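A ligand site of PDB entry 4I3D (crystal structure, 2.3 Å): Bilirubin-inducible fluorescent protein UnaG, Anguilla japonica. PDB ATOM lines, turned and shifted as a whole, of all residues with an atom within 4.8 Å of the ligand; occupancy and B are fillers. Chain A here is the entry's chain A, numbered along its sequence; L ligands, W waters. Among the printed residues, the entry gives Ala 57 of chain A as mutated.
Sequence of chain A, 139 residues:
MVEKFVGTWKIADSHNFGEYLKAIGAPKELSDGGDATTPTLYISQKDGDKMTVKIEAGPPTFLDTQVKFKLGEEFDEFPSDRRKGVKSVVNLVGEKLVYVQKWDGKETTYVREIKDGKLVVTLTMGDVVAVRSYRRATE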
ATOM      1  N   PHE A   5      -9.193 -12.522 -33.273  1.00  0.00           N
ATOM      2  CA  PHE A   5      -9.076 -12.206 -31.850  1.00  0.00           C
ATOM      3  C   PHE A   5      -9.437 -13.386 -30.974  1.00  0.00           C
ATOM      4  O   PHE A   5      -9.115 -13.408 -29.801  1.00  0.00           O
ATOM      5  CB  PHE A   5      -9.999 -11.042 -31.486  1.00  0.00           C
ATOM      6  CG  PHE A   5      -9.524  -9.716 -32.005  1.00  0.00           C
ATOM      7  CD1 PHE A   5      -8.317  -9.191 -31.578  1.00  0.00           C
ATOM      8  CD2 PHE A   5     -10.267  -8.999 -32.907  1.00  0.00           C
ATOM      9  CE1 PHE A   5      -7.877  -7.990 -32.048  1.00  0.00           C
ATOM     10  CE2 PHE A   5      -9.827  -7.798 -33.376  1.00  0.00           C
ATOM     11  CZ  PHE A   5      -8.640  -7.293 -32.941  1.00  0.00           C
ATOM     12  N   PHE A  17       0.370   1.148 -17.557  1.00  0.00           N
ATOM     13  CA  PHE A  17      -1.010   0.722 -17.316  1.00  0.00           C
ATOM     14  C   PHE A  17      -1.508   1.164 -15.945  1.00  0.00           C
ATOM     15  O   PHE A  17      -2.711   1.355 -15.741  1.00  0.00           O
ATOM     16  CB  PHE A  17      -1.129  -0.787 -17.456  1.00  0.00           C
ATOM     17  CG  PHE A  17      -2.532  -1.327 -17.254  1.00  0.00           C
ATOM     18  CD1 PHE A  17      -3.562  -0.964 -18.094  1.00  0.00           C
ATOM     19  CD2 PHE A  17      -2.795  -2.206 -16.235  1.00  0.00           C
ATOM     20  CE1 PHE A  17      -4.839  -1.471 -17.891  1.00  0.00           C
ATOM     21  CE2 PHE A  17      -4.056  -2.715 -16.044  1.00  0.00           C
ATOM     22  CZ  PHE A  17      -5.070  -2.334 -16.862  1.00  0.00           C
ATOM     23  N   TYR A  20      -2.419   4.742 -16.414  1.00  0.00           N
ATOM     24  CA  TYR A  20      -3.648   4.801 -17.157  1.00  0.00           C
ATOM     25  C   TYR A  20      -4.797   4.657 -16.165  1.00  0.00           C
ATOM     26  O   TYR A  20      -5.691   5.497 -16.091  1.00  0.00           O
ATOM     27  CB  TYR A  20      -3.702   3.699 -18.219  1.00  0.00           C
ATOM     28  CG  TYR A  20      -5.098   3.489 -18.720  1.00  0.00           C
ATOM     29  CD1 TYR A  20      -5.672   4.380 -19.607  1.00  0.00           C
ATOM     30  CD2 TYR A  20      -5.880   2.428 -18.263  1.00  0.00           C
ATOM     31  CE1 TYR A  20      -6.970   4.226 -20.044  1.00  0.00           C
ATOM     32  CE2 TYR A  20      -7.189   2.269 -18.715  1.00  0.00           C
ATOM     33  CZ  TYR A  20      -7.722   3.175 -19.598  1.00  0.00           C
ATOM     34  OH  TYR A  20      -9.019   3.054 -20.070  1.00  0.00           O
ATOM     35  N   LEU A  21      -4.745   3.593 -15.357  1.00  0.00           N
ATOM     36  CA  LEU A  21      -5.765   3.322 -14.343  1.00  0.00           C
ATOM     37  C   LEU A  21      -5.913   4.484 -13.382  1.00  0.00           C
ATOM     38  O   LEU A  21      -7.010   4.847 -12.976  1.00  0.00           O
ATOM     39  CB  LEU A  21      -5.432   2.047 -13.585  1.00  0.00           C
ATOM     40  CG  LEU A  21      -5.722   0.764 -14.357  1.00  0.00           C
ATOM     41  CD1 LEU A  21      -5.247  -0.479 -13.609  1.00  0.00           C
ATOM     42  CD2 LEU A  21      -7.220   0.662 -14.665  1.00  0.00           C
ATOM     43  N   ALA A  26      -9.165   5.366 -11.216  1.00  0.00           N
ATOM     44  CA  ALA A  26      -9.174   4.119 -10.460  1.00  0.00           C
ATOM     45  C   ALA A  26      -8.419   4.315  -9.146  1.00  0.00           C
ATOM     46  O   ALA A  26      -7.396   4.991  -9.101  1.00  0.00           O
ATOM     47  CB  ALA A  26      -8.554   2.985 -11.276  1.00  0.00           C
ATOM     48  N   LEU A  30      -5.786  -0.192  -6.486  1.00  0.00           N
ATOM     49  CA  LEU A  30      -6.055  -0.993  -7.675  1.00  0.00           C
ATOM     50  C   LEU A  30      -5.147  -0.580  -8.828  1.00  0.00           C
ATOM     51  O   LEU A  30      -4.849  -1.381  -9.717  1.00  0.00           O
ATOM     52  CB  LEU A  30      -7.513  -0.829  -8.093  1.00  0.00           C
ATOM     53  CG  LEU A  30      -8.517  -1.353  -7.065  1.00  0.00           C
ATOM     54  CD1 LEU A  30      -9.933  -1.080  -7.520  1.00  0.00           C
ATOM     55  CD2 LEU A  30      -8.313  -2.864  -6.815  1.00  0.00           C
ATOM     56  N   THR A  37      -0.089  -6.989 -13.112  1.00  0.00           N
ATOM     57  CA  THR A  37      -1.259  -7.873 -13.189  1.00  0.00           C
ATOM     58  C   THR A  37      -1.179  -8.746 -14.432  1.00  0.00           C
ATOM     59  O   THR A  37      -0.724  -8.301 -15.483  1.00  0.00           O
ATOM     60  CB  THR A  37      -2.574  -7.073 -13.205  1.00  0.00           C
ATOM     61  OG1 THR A  37      -2.685  -6.341 -14.429  1.00  0.00           O
ATOM     62  CG2 THR A  37      -2.634  -6.110 -12.030  1.00  0.00           C
ATOM     63  N   LEU A  41      -7.344 -13.832 -20.942  1.00  0.00           N
ATOM     64  CA  LEU A  41      -8.574 -13.539 -21.692  1.00  0.00           C
ATOM     65  C   LEU A  41      -9.039 -14.764 -22.457  1.00  0.00           C
ATOM     66  O   LEU A  41      -8.231 -15.566 -22.900  1.00  0.00           O
ATOM     67  CB  LEU A  41      -8.321 -12.449 -22.730  1.00  0.00           C
ATOM     68  CG  LEU A  41      -7.577 -11.186 -22.357  1.00  0.00           C
ATOM     69  CD1 LEU A  41      -7.468 -10.311 -23.594  1.00  0.00           C
ATOM     70  CD2 LEU A  41      -8.263 -10.459 -21.229  1.00  0.00           C
ATOM     71  N   ILE A  43     -11.548 -15.369 -25.491  1.00  0.00           N
ATOM     72  CA  ILE A  43     -12.294 -14.615 -26.453  1.00  0.00           C
ATOM     73  C   ILE A  43     -12.943 -15.516 -27.476  1.00  0.00           C
ATOM     74  O   ILE A  43     -12.287 -16.392 -28.040  1.00  0.00           O
ATOM     75  CB  ILE A  43     -11.379 -13.656 -27.180  1.00  0.00           C
ATOM     76  CG1 ILE A  43     -10.504 -12.921 -26.168  1.00  0.00           C
ATOM     77  CG2 ILE A  43     -12.190 -12.706 -28.027  1.00  0.00           C
ATOM     78  CD1 ILE A  43      -9.660 -11.865 -26.797  1.00  0.00           C
ATOM     79  N   MET A  51     -19.579 -10.743 -29.795  1.00  0.00           N
ATOM     80  CA  MET A  51     -18.380 -11.256 -29.171  1.00  0.00           C
ATOM     81  C   MET A  51     -18.626 -11.470 -27.706  1.00  0.00           C
ATOM     82  O   MET A  51     -19.510 -10.850 -27.127  1.00  0.00           O
ATOM     83  CB  MET A  51     -17.235 -10.270 -29.349  1.00  0.00           C
ATOM     84  CG  MET A  51     -16.678 -10.265 -30.734  1.00  0.00           C
ATOM     85  SD  MET A  51     -15.321  -9.100 -30.941  1.00  0.00           S
ATOM     86  CE  MET A  51     -14.117  -9.750 -29.809  1.00  0.00           C
ATOM     87  N   VAL A  53     -16.153 -12.127 -24.057  1.00  0.00           N
ATOM     88  CA  VAL A  53     -14.779 -12.160 -23.529  1.00  0.00           C
ATOM     89  C   VAL A  53     -14.819 -12.423 -22.045  1.00  0.00           C
ATOM     90  O   VAL A  53     -15.304 -11.615 -21.266  1.00  0.00           O
ATOM     91  CB  VAL A  53     -14.035 -10.830 -23.788  1.00  0.00           C
ATOM     92  CG1 VAL A  53     -12.553 -10.924 -23.345  1.00  0.00           C
ATOM     93  CG2 VAL A  53     -14.115 -10.448 -25.246  1.00  0.00           C
ATOM     94  N   ILE A  55     -12.584 -12.912 -18.682  1.00  0.00           N
ATOM     95  CA  ILE A  55     -11.305 -12.492 -18.160  1.00  0.00           C
ATOM     96  C   ILE A  55     -11.080 -13.168 -16.832  1.00  0.00           C
ATOM     97  O   ILE A  55     -11.960 -13.130 -15.963  1.00  0.00           O
ATOM     98  CB  ILE A  55     -11.266 -10.978 -17.925  1.00  0.00           C
ATOM     99  CG1 ILE A  55     -11.577 -10.230 -19.225  1.00  0.00           C
ATOM    100  CG2 ILE A  55      -9.917 -10.557 -17.390  1.00  0.00           C
ATOM    101  CD1 ILE A  55     -13.054  -9.947 -19.437  1.00  0.00           C
ATOM    102  N   ALA A  57      -8.868 -12.449 -13.935  1.00  0.00           N
ATOM    103  CA  ALA A  57      -8.045 -11.318 -13.541  1.00  0.00           C
ATOM    104  C   ALA A  57      -6.734 -11.765 -12.904  1.00  0.00           C
ATOM    105  O   ALA A  57      -5.734 -11.039 -12.948  1.00  0.00           O
ATOM    106  CB  ALA A  57      -8.817 -10.401 -12.624  1.00  0.00           C
ATOM    107  N   THR A  61      -6.432 -10.107  -6.567  1.00  0.00           N
ATOM    108  CA  THR A  61      -7.854  -9.946  -6.272  1.00  0.00           C
ATOM    109  C   THR A  61      -8.781 -10.939  -7.002  1.00  0.00           C
ATOM    110  O   THR A  61      -9.877 -11.195  -6.549  1.00  0.00           O
ATOM    111  CB  THR A  61      -8.325  -8.546  -6.663  1.00  0.00           C
ATOM    112  OG1 THR A  61      -7.863  -8.260  -8.002  1.00  0.00           O
ATOM    113  CG2 THR A  61      -7.773  -7.511  -5.738  1.00  0.00           C
ATOM    114  N   LEU A  63     -10.551 -10.537  -9.696  1.00  0.00           N
ATOM    115  CA  LEU A  63     -11.788  -9.873 -10.058  1.00  0.00           C
ATOM    116  C   LEU A  63     -12.257 -10.374 -11.422  1.00  0.00           C
ATOM    117  O   LEU A  63     -12.389  -9.588 -12.368  1.00  0.00           O
ATOM    118  CB  LEU A  63     -11.556  -8.362 -10.089  1.00  0.00           C
ATOM    119  CG  LEU A  63     -11.136  -7.729  -8.755  1.00  0.00           C
ATOM    120  CD1 LEU A  63     -10.772  -6.264  -8.906  1.00  0.00           C
ATOM    121  CD2 LEU A  63     -12.251  -7.893  -7.730  1.00  0.00           C
ATOM    122  N   THR A  65     -14.326 -11.754 -14.642  1.00  0.00           N
ATOM    123  CA  THR A  65     -15.551 -11.203 -15.219  1.00  0.00           C
ATOM    124  C   THR A  65     -15.814 -11.667 -16.643  1.00  0.00           C
ATOM    125  O   THR A  65     -15.111 -12.516 -17.161  1.00  0.00           O
ATOM    126  CB  THR A  65     -15.498  -9.654 -15.195  1.00  0.00           C
ATOM    127  OG1 THR A  65     -16.440  -9.124 -16.151  1.00  0.00           O
ATOM    128  CG2 THR A  65     -14.095  -9.178 -15.494  1.00  0.00           C
ATOM    129  N   VAL A  67     -17.613  -9.904 -20.559  1.00  0.00           N
ATOM    130  CA  VAL A  67     -18.464  -8.950 -21.289  1.00  0.00           C
ATOM    131  C   VAL A  67     -18.979  -9.563 -22.586  1.00  0.00           C
ATOM    132  O   VAL A  67     -18.295 -10.350 -23.224  1.00  0.00           O
ATOM    133  CB  VAL A  67     -17.740  -7.640 -21.628  1.00  0.00           C
ATOM    134  CG1 VAL A  67     -17.420  -6.878 -20.362  1.00  0.00           C
ATOM    135  CG2 VAL A  67     -16.468  -7.927 -22.438  1.00  0.00           C
ATOM    136  N   PHE A  69     -21.140  -8.448 -26.169  1.00  0.00           N
ATOM    137  CA  PHE A  69     -21.665  -7.331 -26.905  1.00  0.00           C
ATOM    138  C   PHE A  69     -21.912  -7.665 -28.354  1.00  0.00           C
ATOM    139  O   PHE A  69     -21.554  -8.735 -28.835  1.00  0.00           O
ATOM    140  CB  PHE A  69     -20.724  -6.137 -26.819  1.00  0.00           C
ATOM    141  CG  PHE A  69     -19.284  -6.449 -27.196  1.00  0.00           C
ATOM    142  CD1 PHE A  69     -18.873  -6.411 -28.511  1.00  0.00           C
ATOM    143  CD2 PHE A  69     -18.350  -6.790 -26.217  1.00  0.00           C
ATOM    144  CE1 PHE A  69     -17.563  -6.706 -28.849  1.00  0.00           C
ATOM    145  CE2 PHE A  69     -17.041  -7.085 -26.555  1.00  0.00           C
ATOM    146  CZ  PHE A  69     -16.651  -7.047 -27.867  1.00  0.00           C
ATOM    147  N   GLU A  77     -21.584  -1.420 -18.766  1.00  0.00           N
ATOM    148  CA  GLU A  77     -20.484  -2.186 -18.172  1.00  0.00           C
ATOM    149  C   GLU A  77     -20.334  -1.872 -16.684  1.00  0.00           C
ATOM    150  O   GLU A  77     -20.793  -0.837 -16.222  1.00  0.00           O
ATOM    151  CB  GLU A  77     -19.167  -1.923 -18.902  1.00  0.00           C
ATOM    152  CG  GLU A  77     -18.086  -2.976 -18.601  1.00  0.00           C
ATOM    153  CD  GLU A  77     -16.795  -2.789 -19.379  1.00  0.00           C
ATOM    154  OE1 GLU A  77     -16.775  -2.019 -20.366  1.00  0.00           O
ATOM    155  OE2 GLU A  77     -15.789  -3.418 -19.000  1.00  0.00           O
ATOM    156  N   PRO A  79     -17.113  -2.185 -14.548  1.00  0.00           N
ATOM    157  CA  PRO A  79     -15.659  -2.403 -14.531  1.00  0.00           C
ATOM    158  C   PRO A  79     -15.021  -2.595 -13.153  1.00  0.00           C
ATOM    159  O   PRO A  79     -15.443  -2.003 -12.176  1.00  0.00           O
ATOM    160  CB  PRO A  79     -15.095  -1.126 -15.164  1.00  0.00           C
ATOM    161  CG  PRO A  79     -16.275  -0.453 -15.811  1.00  0.00           C
ATOM    162  CD  PRO A  79     -17.447  -0.836 -15.036  1.00  0.00           C
ATOM    163  N   SER A  80     -13.963  -3.384 -13.120  1.00  0.00           N
ATOM    164  CA  SER A  80     -13.233  -3.656 -11.899  1.00  0.00           C
ATOM    165  C   SER A  80     -12.859  -2.356 -11.219  1.00  0.00           C
ATOM    166  O   SER A  80     -12.907  -2.257  -9.992  1.00  0.00           O
ATOM    167  CB  SER A  80     -11.975  -4.484 -12.203  1.00  0.00           C
ATOM    168  OG  SER A  80     -12.316  -5.700 -12.844  1.00  0.00           O
ATOM    169  N   ASP A  81     -12.502  -1.353 -12.013  1.00  0.00           N
ATOM    170  CA  ASP A  81     -11.908  -0.145 -11.464  1.00  0.00           C
ATOM    171  C   ASP A  81     -12.905   0.701 -10.668  1.00  0.00           C
ATOM    172  O   ASP A  81     -12.528   1.728 -10.096  1.00  0.00           O
ATOM    173  CB  ASP A  81     -11.285   0.684 -12.576  1.00  0.00           C
ATOM    174  CG  ASP A  81     -12.162   0.801 -13.782  1.00  0.00           C
ATOM    175  OD1 ASP A  81     -13.120   1.599 -13.726  1.00  0.00           O
ATOM    176  OD2 ASP A  81     -11.916   0.075 -14.769  1.00  0.00           O
ATOM    177  N   LEU A  97     -10.051  -3.218 -33.683  1.00  0.00           N
ATOM    178  CA  LEU A  97     -11.271  -3.146 -32.883  1.00  0.00           C
ATOM    179  C   LEU A  97     -11.203  -1.949 -31.949  1.00  0.00           C
ATOM    180  O   LEU A  97     -10.187  -1.718 -31.294  1.00  0.00           O
ATOM    181  CB  LEU A  97     -11.392  -4.431 -32.073  1.00  0.00           C
ATOM    182  CG  LEU A  97     -12.747  -4.722 -31.446  1.00  0.00           C
ATOM    183  CD1 LEU A  97     -13.791  -4.973 -32.522  1.00  0.00           C
ATOM    184  CD2 LEU A  97     -12.597  -5.928 -30.538  1.00  0.00           C
ATOM    185  N   TYR A  99     -12.992   0.239 -28.775  1.00  0.00           N
ATOM    186  CA  TYR A  99     -13.843   0.015 -27.631  1.00  0.00           C
ATOM    187  C   TYR A  99     -13.931   1.357 -26.933  1.00  0.00           C
ATOM    188  O   TYR A  99     -12.906   1.905 -26.558  1.00  0.00           O
ATOM    189  CB  TYR A  99     -13.150  -0.994 -26.719  1.00  0.00           C
ATOM    190  CG  TYR A  99     -14.016  -1.690 -25.687  1.00  0.00           C
ATOM    191  CD1 TYR A  99     -14.456  -1.030 -24.551  1.00  0.00           C
ATOM    192  CD2 TYR A  99     -14.331  -3.032 -25.825  1.00  0.00           C
ATOM    193  CE1 TYR A  99     -15.224  -1.682 -23.592  1.00  0.00           C
ATOM    194  CE2 TYR A  99     -15.096  -3.687 -24.880  1.00  0.00           C
ATOM    195  CZ  TYR A  99     -15.542  -3.004 -23.772  1.00  0.00           C
ATOM    196  OH  TYR A  99     -16.306  -3.668 -22.824  1.00  0.00           O
ATOM    197  N   TYR A 110     -10.058   2.108 -26.065  1.00  0.00           N
ATOM    198  CA  TYR A 110      -9.195   0.920 -26.112  1.00  0.00           C
ATOM    199  C   TYR A 110      -9.095   0.464 -27.560  1.00  0.00           C
ATOM    200  O   TYR A 110     -10.107   0.142 -28.165  1.00  0.00           O
ATOM    201  CB  TYR A 110      -9.798  -0.259 -25.353  1.00  0.00           C
ATOM    202  CG  TYR A 110     -10.154  -0.002 -23.901  1.00  0.00           C
ATOM    203  CD1 TYR A 110     -11.334   0.618 -23.552  1.00  0.00           C
ATOM    204  CD2 TYR A 110      -9.315  -0.417 -22.894  1.00  0.00           C
ATOM    205  CE1 TYR A 110     -11.667   0.839 -22.220  1.00  0.00           C
ATOM    206  CE2 TYR A 110      -9.632  -0.197 -21.573  1.00  0.00           C
ATOM    207  CZ  TYR A 110     -10.810   0.419 -21.238  1.00  0.00           C
ATOM    208  OH  TYR A 110     -11.120   0.632 -19.907  1.00  0.00           O
ATOM    209  N   ARG A 112      -7.543  -2.403 -30.063  1.00  0.00           N
ATOM    210  CA  ARG A 112      -6.930  -3.716 -30.017  1.00  0.00           C
ATOM    211  C   ARG A 112      -6.685  -4.222 -31.428  1.00  0.00           C
ATOM    212  O   ARG A 112      -7.499  -4.032 -32.308  1.00  0.00           O
ATOM    213  CB  ARG A 112      -7.866  -4.651 -29.269  1.00  0.00           C
ATOM    214  CG  ARG A 112      -8.008  -4.261 -27.822  1.00  0.00           C
ATOM    215  CD  ARG A 112      -8.896  -5.215 -27.091  1.00  0.00           C
ATOM    216  NE  ARG A 112      -8.918  -4.960 -25.651  1.00  0.00           N
ATOM    217  CZ  ARG A 112      -9.827  -4.216 -25.015  1.00  0.00           C
ATOM    218  NH1 ARG A 112     -10.799  -3.612 -25.691  1.00  0.00           N
ATOM    219  NH2 ARG A 112      -9.755  -4.077 -23.710  1.00  0.00           N
ATOM    220  N   LEU A 119      -1.846 -10.044 -29.330  1.00  0.00           N
ATOM    221  CA  LEU A 119      -3.025  -9.187 -29.246  1.00  0.00           C
ATOM    222  C   LEU A 119      -2.621  -7.911 -28.504  1.00  0.00           C
ATOM    223  O   LEU A 119      -2.341  -7.955 -27.319  1.00  0.00           O
ATOM    224  CB  LEU A 119      -4.159  -9.899 -28.524  1.00  0.00           C
ATOM    225  CG  LEU A 119      -5.514  -9.195 -28.622  1.00  0.00           C
ATOM    226  CD1 LEU A 119      -6.618 -10.240 -28.711  1.00  0.00           C
ATOM    227  CD2 LEU A 119      -5.720  -8.286 -27.439  1.00  0.00           C
ATOM    228  N   VAL A 121      -3.139  -3.940 -27.253  1.00  0.00           N
ATOM    229  CA  VAL A 121      -4.189  -3.015 -26.888  1.00  0.00           C
ATOM    230  C   VAL A 121      -3.545  -1.750 -26.379  1.00  0.00           C
ATOM    231  O   VAL A 121      -2.684  -1.785 -25.517  1.00  0.00           O
ATOM    232  CB  VAL A 121      -5.135  -3.560 -25.794  1.00  0.00           C
ATOM    233  CG1 VAL A 121      -4.365  -4.016 -24.584  1.00  0.00           C
ATOM    234  CG2 VAL A 121      -6.147  -2.486 -25.425  1.00  0.00           C
ATOM    235  N   LEU A 123      -4.394   1.739 -24.627  1.00  0.00           N
ATOM    236  CA  LEU A 123      -5.424   2.371 -23.806  1.00  0.00           C
ATOM    237  C   LEU A 123      -5.183   3.882 -23.754  1.00  0.00           C
ATOM    238  O   LEU A 123      -4.075   4.334 -23.512  1.00  0.00           O
ATOM    239  CB  LEU A 123      -5.377   1.801 -22.393  1.00  0.00           C
ATOM    240  CG  LEU A 123      -5.327   0.262 -22.290  1.00  0.00           C
ATOM    241  CD1 LEU A 123      -3.878  -0.308 -22.315  1.00  0.00           C
ATOM    242  CD2 LEU A 123      -6.054  -0.162 -21.036  1.00  0.00           C
ATOM    243  N   ARG A 132      -0.467  -2.667 -23.637  1.00  0.00           N
ATOM    244  CA  ARG A 132      -0.261  -4.011 -23.122  1.00  0.00           C
ATOM    245  C   ARG A 132      -0.371  -4.990 -24.295  1.00  0.00           C
ATOM    246  O   ARG A 132      -1.119  -4.738 -25.242  1.00  0.00           O
ATOM    247  CB  ARG A 132      -1.324  -4.321 -22.078  1.00  0.00           C
ATOM    248  CG  ARG A 132      -1.252  -3.419 -20.865  1.00  0.00           C
ATOM    249  CD  ARG A 132      -2.298  -3.792 -19.878  1.00  0.00           C
ATOM    250  NE  ARG A 132      -1.738  -4.597 -18.792  1.00  0.00           N
ATOM    251  CZ  ARG A 132      -2.469  -5.352 -17.980  1.00  0.00           C
ATOM    252  NH1 ARG A 132      -3.796  -5.409 -18.120  1.00  0.00           N
ATOM    253  NH2 ARG A 132      -1.887  -6.053 -17.031  1.00  0.00           N
ATOM    254  N   TYR A 134      -0.562  -9.284 -25.493  1.00  0.00           N
ATOM    255  CA  TYR A 134      -0.857 -10.613 -25.013  1.00  0.00           C
ATOM    256  C   TYR A 134      -0.289 -11.571 -26.024  1.00  0.00           C
ATOM    257  O   TYR A 134      -0.308 -11.290 -27.228  1.00  0.00           O
ATOM    258  CB  TYR A 134      -2.366 -10.853 -24.940  1.00  0.00           C
ATOM    259  CG  TYR A 134      -3.091 -10.109 -23.852  1.00  0.00           C
ATOM    260  CD1 TYR A 134      -3.431  -8.783 -23.998  1.00  0.00           C
ATOM    261  CD2 TYR A 134      -3.473 -10.756 -22.678  1.00  0.00           C
ATOM    262  CE1 TYR A 134      -4.119  -8.099 -23.008  1.00  0.00           C
ATOM    263  CE2 TYR A 134      -4.166 -10.084 -21.693  1.00  0.00           C
ATOM    264  CZ  TYR A 134      -4.482  -8.750 -21.858  1.00  0.00           C
ATOM    265  OH  TYR A 134      -5.165  -8.064 -20.860  1.00  0.00           O
HETATM  266  C1  LIG L   1      -8.768  -6.550 -19.065  1.00  0.00           C
HETATM  267  N1  LIG L   1     -10.144  -6.730 -21.194  1.00  0.00           N
HETATM  268  C2  LIG L   1     -10.048  -6.616 -19.834  1.00  0.00           C
HETATM  269  C3  LIG L   1     -11.341  -6.528 -19.330  1.00  0.00           C
HETATM  270  C4  LIG L   1     -12.210  -6.602 -20.383  1.00  0.00           C
HETATM  271  C5  LIG L   1     -11.457  -6.718 -21.530  1.00  0.00           C
HETATM  272  C6  LIG L   1     -13.696  -6.554 -20.324  1.00  0.00           C
HETATM  273  C7  LIG L   1     -11.779  -6.397 -17.895  1.00  0.00           C
HETATM  274  C8  LIG L   1     -12.006  -4.973 -17.541  1.00  0.00           C
HETATM  275  C9  LIG L   1     -12.847  -4.921 -16.323  1.00  0.00           C
HETATM  276  O1  LIG L   1     -12.900  -5.909 -15.551  1.00  0.00           O
HETATM  277  O2  LIG L   1     -13.506  -3.899 -16.056  1.00  0.00           O
HETATM  278  C10 LIG L   1     -12.036  -6.817 -22.899  1.00  0.00           C
HETATM  279  N2  LIG L   1      -9.911  -7.581 -24.067  1.00  0.00           N
HETATM  280  C11 LIG L   1     -11.314  -7.202 -23.992  1.00  0.00           C
HETATM  281  C12 LIG L   1     -11.811  -7.227 -25.253  1.00  0.00           C
HETATM  282  C13 LIG L   1     -11.005  -7.590 -26.109  1.00  0.00           C
HETATM  283  C14 LIG L   1      -9.609  -7.891 -25.591  1.00  0.00           C
HETATM  284  C15 LIG L   1     -13.230  -6.861 -25.531  1.00  0.00           C
HETATM  285  O3  LIG L   1      -8.575  -8.262 -26.139  1.00  0.00           O
HETATM  286  C16 LIG L   1     -11.366  -7.675 -27.552  1.00  0.00           C
HETATM  287  C17 LIG L   1     -10.830  -8.628 -28.349  1.00  0.00           C
HETATM  288  N3  LIG L   1      -7.212  -5.173 -14.556  1.00  0.00           N
HETATM  289  C18 LIG L   1      -6.816  -5.657 -13.093  1.00  0.00           C
HETATM  290  C19 LIG L   1      -7.531  -4.546 -12.340  1.00  0.00           C
HETATM  291  C20 LIG L   1      -8.108  -3.727 -13.050  1.00  0.00           C
HETATM  292  C21 LIG L   1      -8.004  -3.968 -14.375  1.00  0.00           C
HETATM  293  C22 LIG L   1      -7.537  -4.466 -10.859  1.00  0.00           C
HETATM  294  O4  LIG L   1      -6.153  -6.622 -12.732  1.00  0.00           O
HETATM  295  C23 LIG L   1      -8.878  -2.583 -12.484  1.00  0.00           C
HETATM  296  C24 LIG L   1      -8.225  -1.528 -11.906  1.00  0.00           C
HETATM  297  C25 LIG L   1      -8.544  -3.237 -15.390  1.00  0.00           C
HETATM  298  N4  LIG L   1      -8.639  -5.170 -16.984  1.00  0.00           N
HETATM  299  C26 LIG L   1      -8.597  -3.850 -16.743  1.00  0.00           C
HETATM  300  C27 LIG L   1      -8.633  -3.134 -18.067  1.00  0.00           C
HETATM  301  C28 LIG L   1      -8.668  -4.047 -19.036  1.00  0.00           C
HETATM  302  C29 LIG L   1      -8.670  -5.356 -18.419  1.00  0.00           C
HETATM  303  C30 LIG L   1      -8.569  -1.663 -18.245  1.00  0.00           C
HETATM  304  C31 LIG L   1      -8.692  -3.756 -20.507  1.00  0.00           C
HETATM  305  C32 LIG L   1      -7.309  -3.686 -21.073  1.00  0.00           C
HETATM  306  C33 LIG L   1      -6.896  -5.026 -21.588  1.00  0.00           C
HETATM  307  O5  LIG L   1      -5.835  -5.561 -21.176  1.00  0.00           O
HETATM  308  O6  LIG L   1      -7.603  -5.617 -22.447  1.00  0.00           O
HETATM  309  O   HOH W   1     -12.121  -1.332 -17.983  1.00  0.00           O
HETATM  310  O   HOH W   2      -4.337  -3.364 -12.079  1.00  0.00           O
HETATM  311  O   HOH W   3     -16.436  -5.370 -16.383  1.00  0.00           O
HETATM  312  O   HOH W   4      -5.312  -6.311 -16.389  1.00  0.00           O
HETATM  313  O   HOH W   5      -8.676  -7.634 -15.607  1.00  0.00           O
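Water W4 lies within hydrogen-bond range of the guanidinium group (NH1) of Arg 132, a nitrogen (N3) of the ligand and the side-chain hydroxyl (OG1) of Thr 37. Water W3 bridges an oxygen (O2) of the ligand (3.3 Å) and the side-chain carboxylate of Glu 77 (3.3 Å). Water W1 lies within hydrogen-bond range of OH of Tyr 110 (2.9 Å) and O2 of the ligand (3.5 Å).
The guanidinium group (NH2) of Arg 112 lies within salt-bridge range of an oxygen (O6) of the ligand. The backbone NH (N) of Ser 80 sits at hydrogen-bond distance from an oxygen (O2) of the ligand, 3.0 Å away. The side-chain hydroxyl (OH) of Tyr 134 sits at hydrogen-bond distance from an oxygen (O5) of the ligand (2.6 Å). The side-chain hydroxyl (OG) of Ser 80 is in hydrogen-bond range of an oxygen (O1) of the ligand, 2.8 Å away. An oxygen (O5) of the ligand lies within salt-bridge range of the guanidinium group of Arg 132, 3.7 Å away.
The side-chain hydroxyl of Tyr 110 lies within hydrogen-bond range of the side-chain hydroxyl of Tyr 20 (3.2 Å). The backbone carbonyl oxygen (O) of Leu 119 lies within hydrogen-bond range of the backbone NH (N) of Tyr 134 (2.9 Å). N of Ile 55 sits at hydrogen-bond distance from O of Thr 65, 3.0 Å away. The backbone carbonyl oxygen of Val 67 is in hydrogen-bond range of the backbone NH of Val 53 (2.9 Å). The backbone carbonyl oxygen (O) of Tyr 99 sits at hydrogen-bond distance from the backbone NH (N) of Tyr 110 (2.9 Å). The backbone carbonyl oxygen (O) of Leu 97 is in hydrogen-bond range of the backbone NH (N) of Arg 112, at 3.0 Å. O of Leu 21 sits at hydrogen-bond distance from N of Ala 26. O of Arg 132 is in hydrogen-bond range of N of Val 121.
CE1 of Phe 17 touches C30 of the ligand, at 3.8 Å. Leu 21 touches the ligand. Leu 30 touches the ligand (CB to C24, 3.9 Å). Thr 37 touches the ligand (CG2 to O4, 3.6 Å). Leu 41 touches the ligand (CD1 to O3, 3.4 Å). Ile 43 touches the ligand. Met 51 touches the ligand. Val 53 touches the ligand. Ile 55 touches the ligand. Thr 65 touches the ligand (CG2 to O1, 3.5 Å). CG1 of Val 67 touches C6 of the ligand, 3.7 Å away. Phe 69 touches the ligand (CE2 to C15, 3.95 Å). OE2 of Glu 77 touches O2 of the ligand, 3.8 Å away. CA of Pro 79 touches O2 of the ligand, 3.0 Å away. Asp 81 touches the ligand. Leu 97 touches the ligand (CD2 to C16, 3.7 Å). Tyr 99 touches the ligand. CE2 of Tyr 110 touches C30 of the ligand, at 3.8 Å. Leu 119 touches the ligand (CD2 to O3, 3.1 Å). Leu 123 touches the ligand (CD2 to C32, 3.7 Å). Hydrophobic or aromatic side chains that line the ligand: Phe 17, Leu 21, Leu 30, Leu 41, Ile 43, Met 51, Val 53, Ile 55, Val 67, Phe 69, Pro 79, Leu 97, Tyr 99, Tyr 110, Leu 119, Leu 123 and Tyr 134. 24 residues have an atom within 4 Å of the ligand: Phe 17, Leu 21, Leu 30, Thr 37, Leu 41, Ile 43, Met 51, Val 53, Ile 55, Thr 65, Val 67, Phe 69, Glu 77, Pro 79, Ser 80, Asp 81, Leu 97, Tyr 99, Tyr 110, Arg 112, Leu 119, Leu 123, Arg 132 and Tyr 134.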
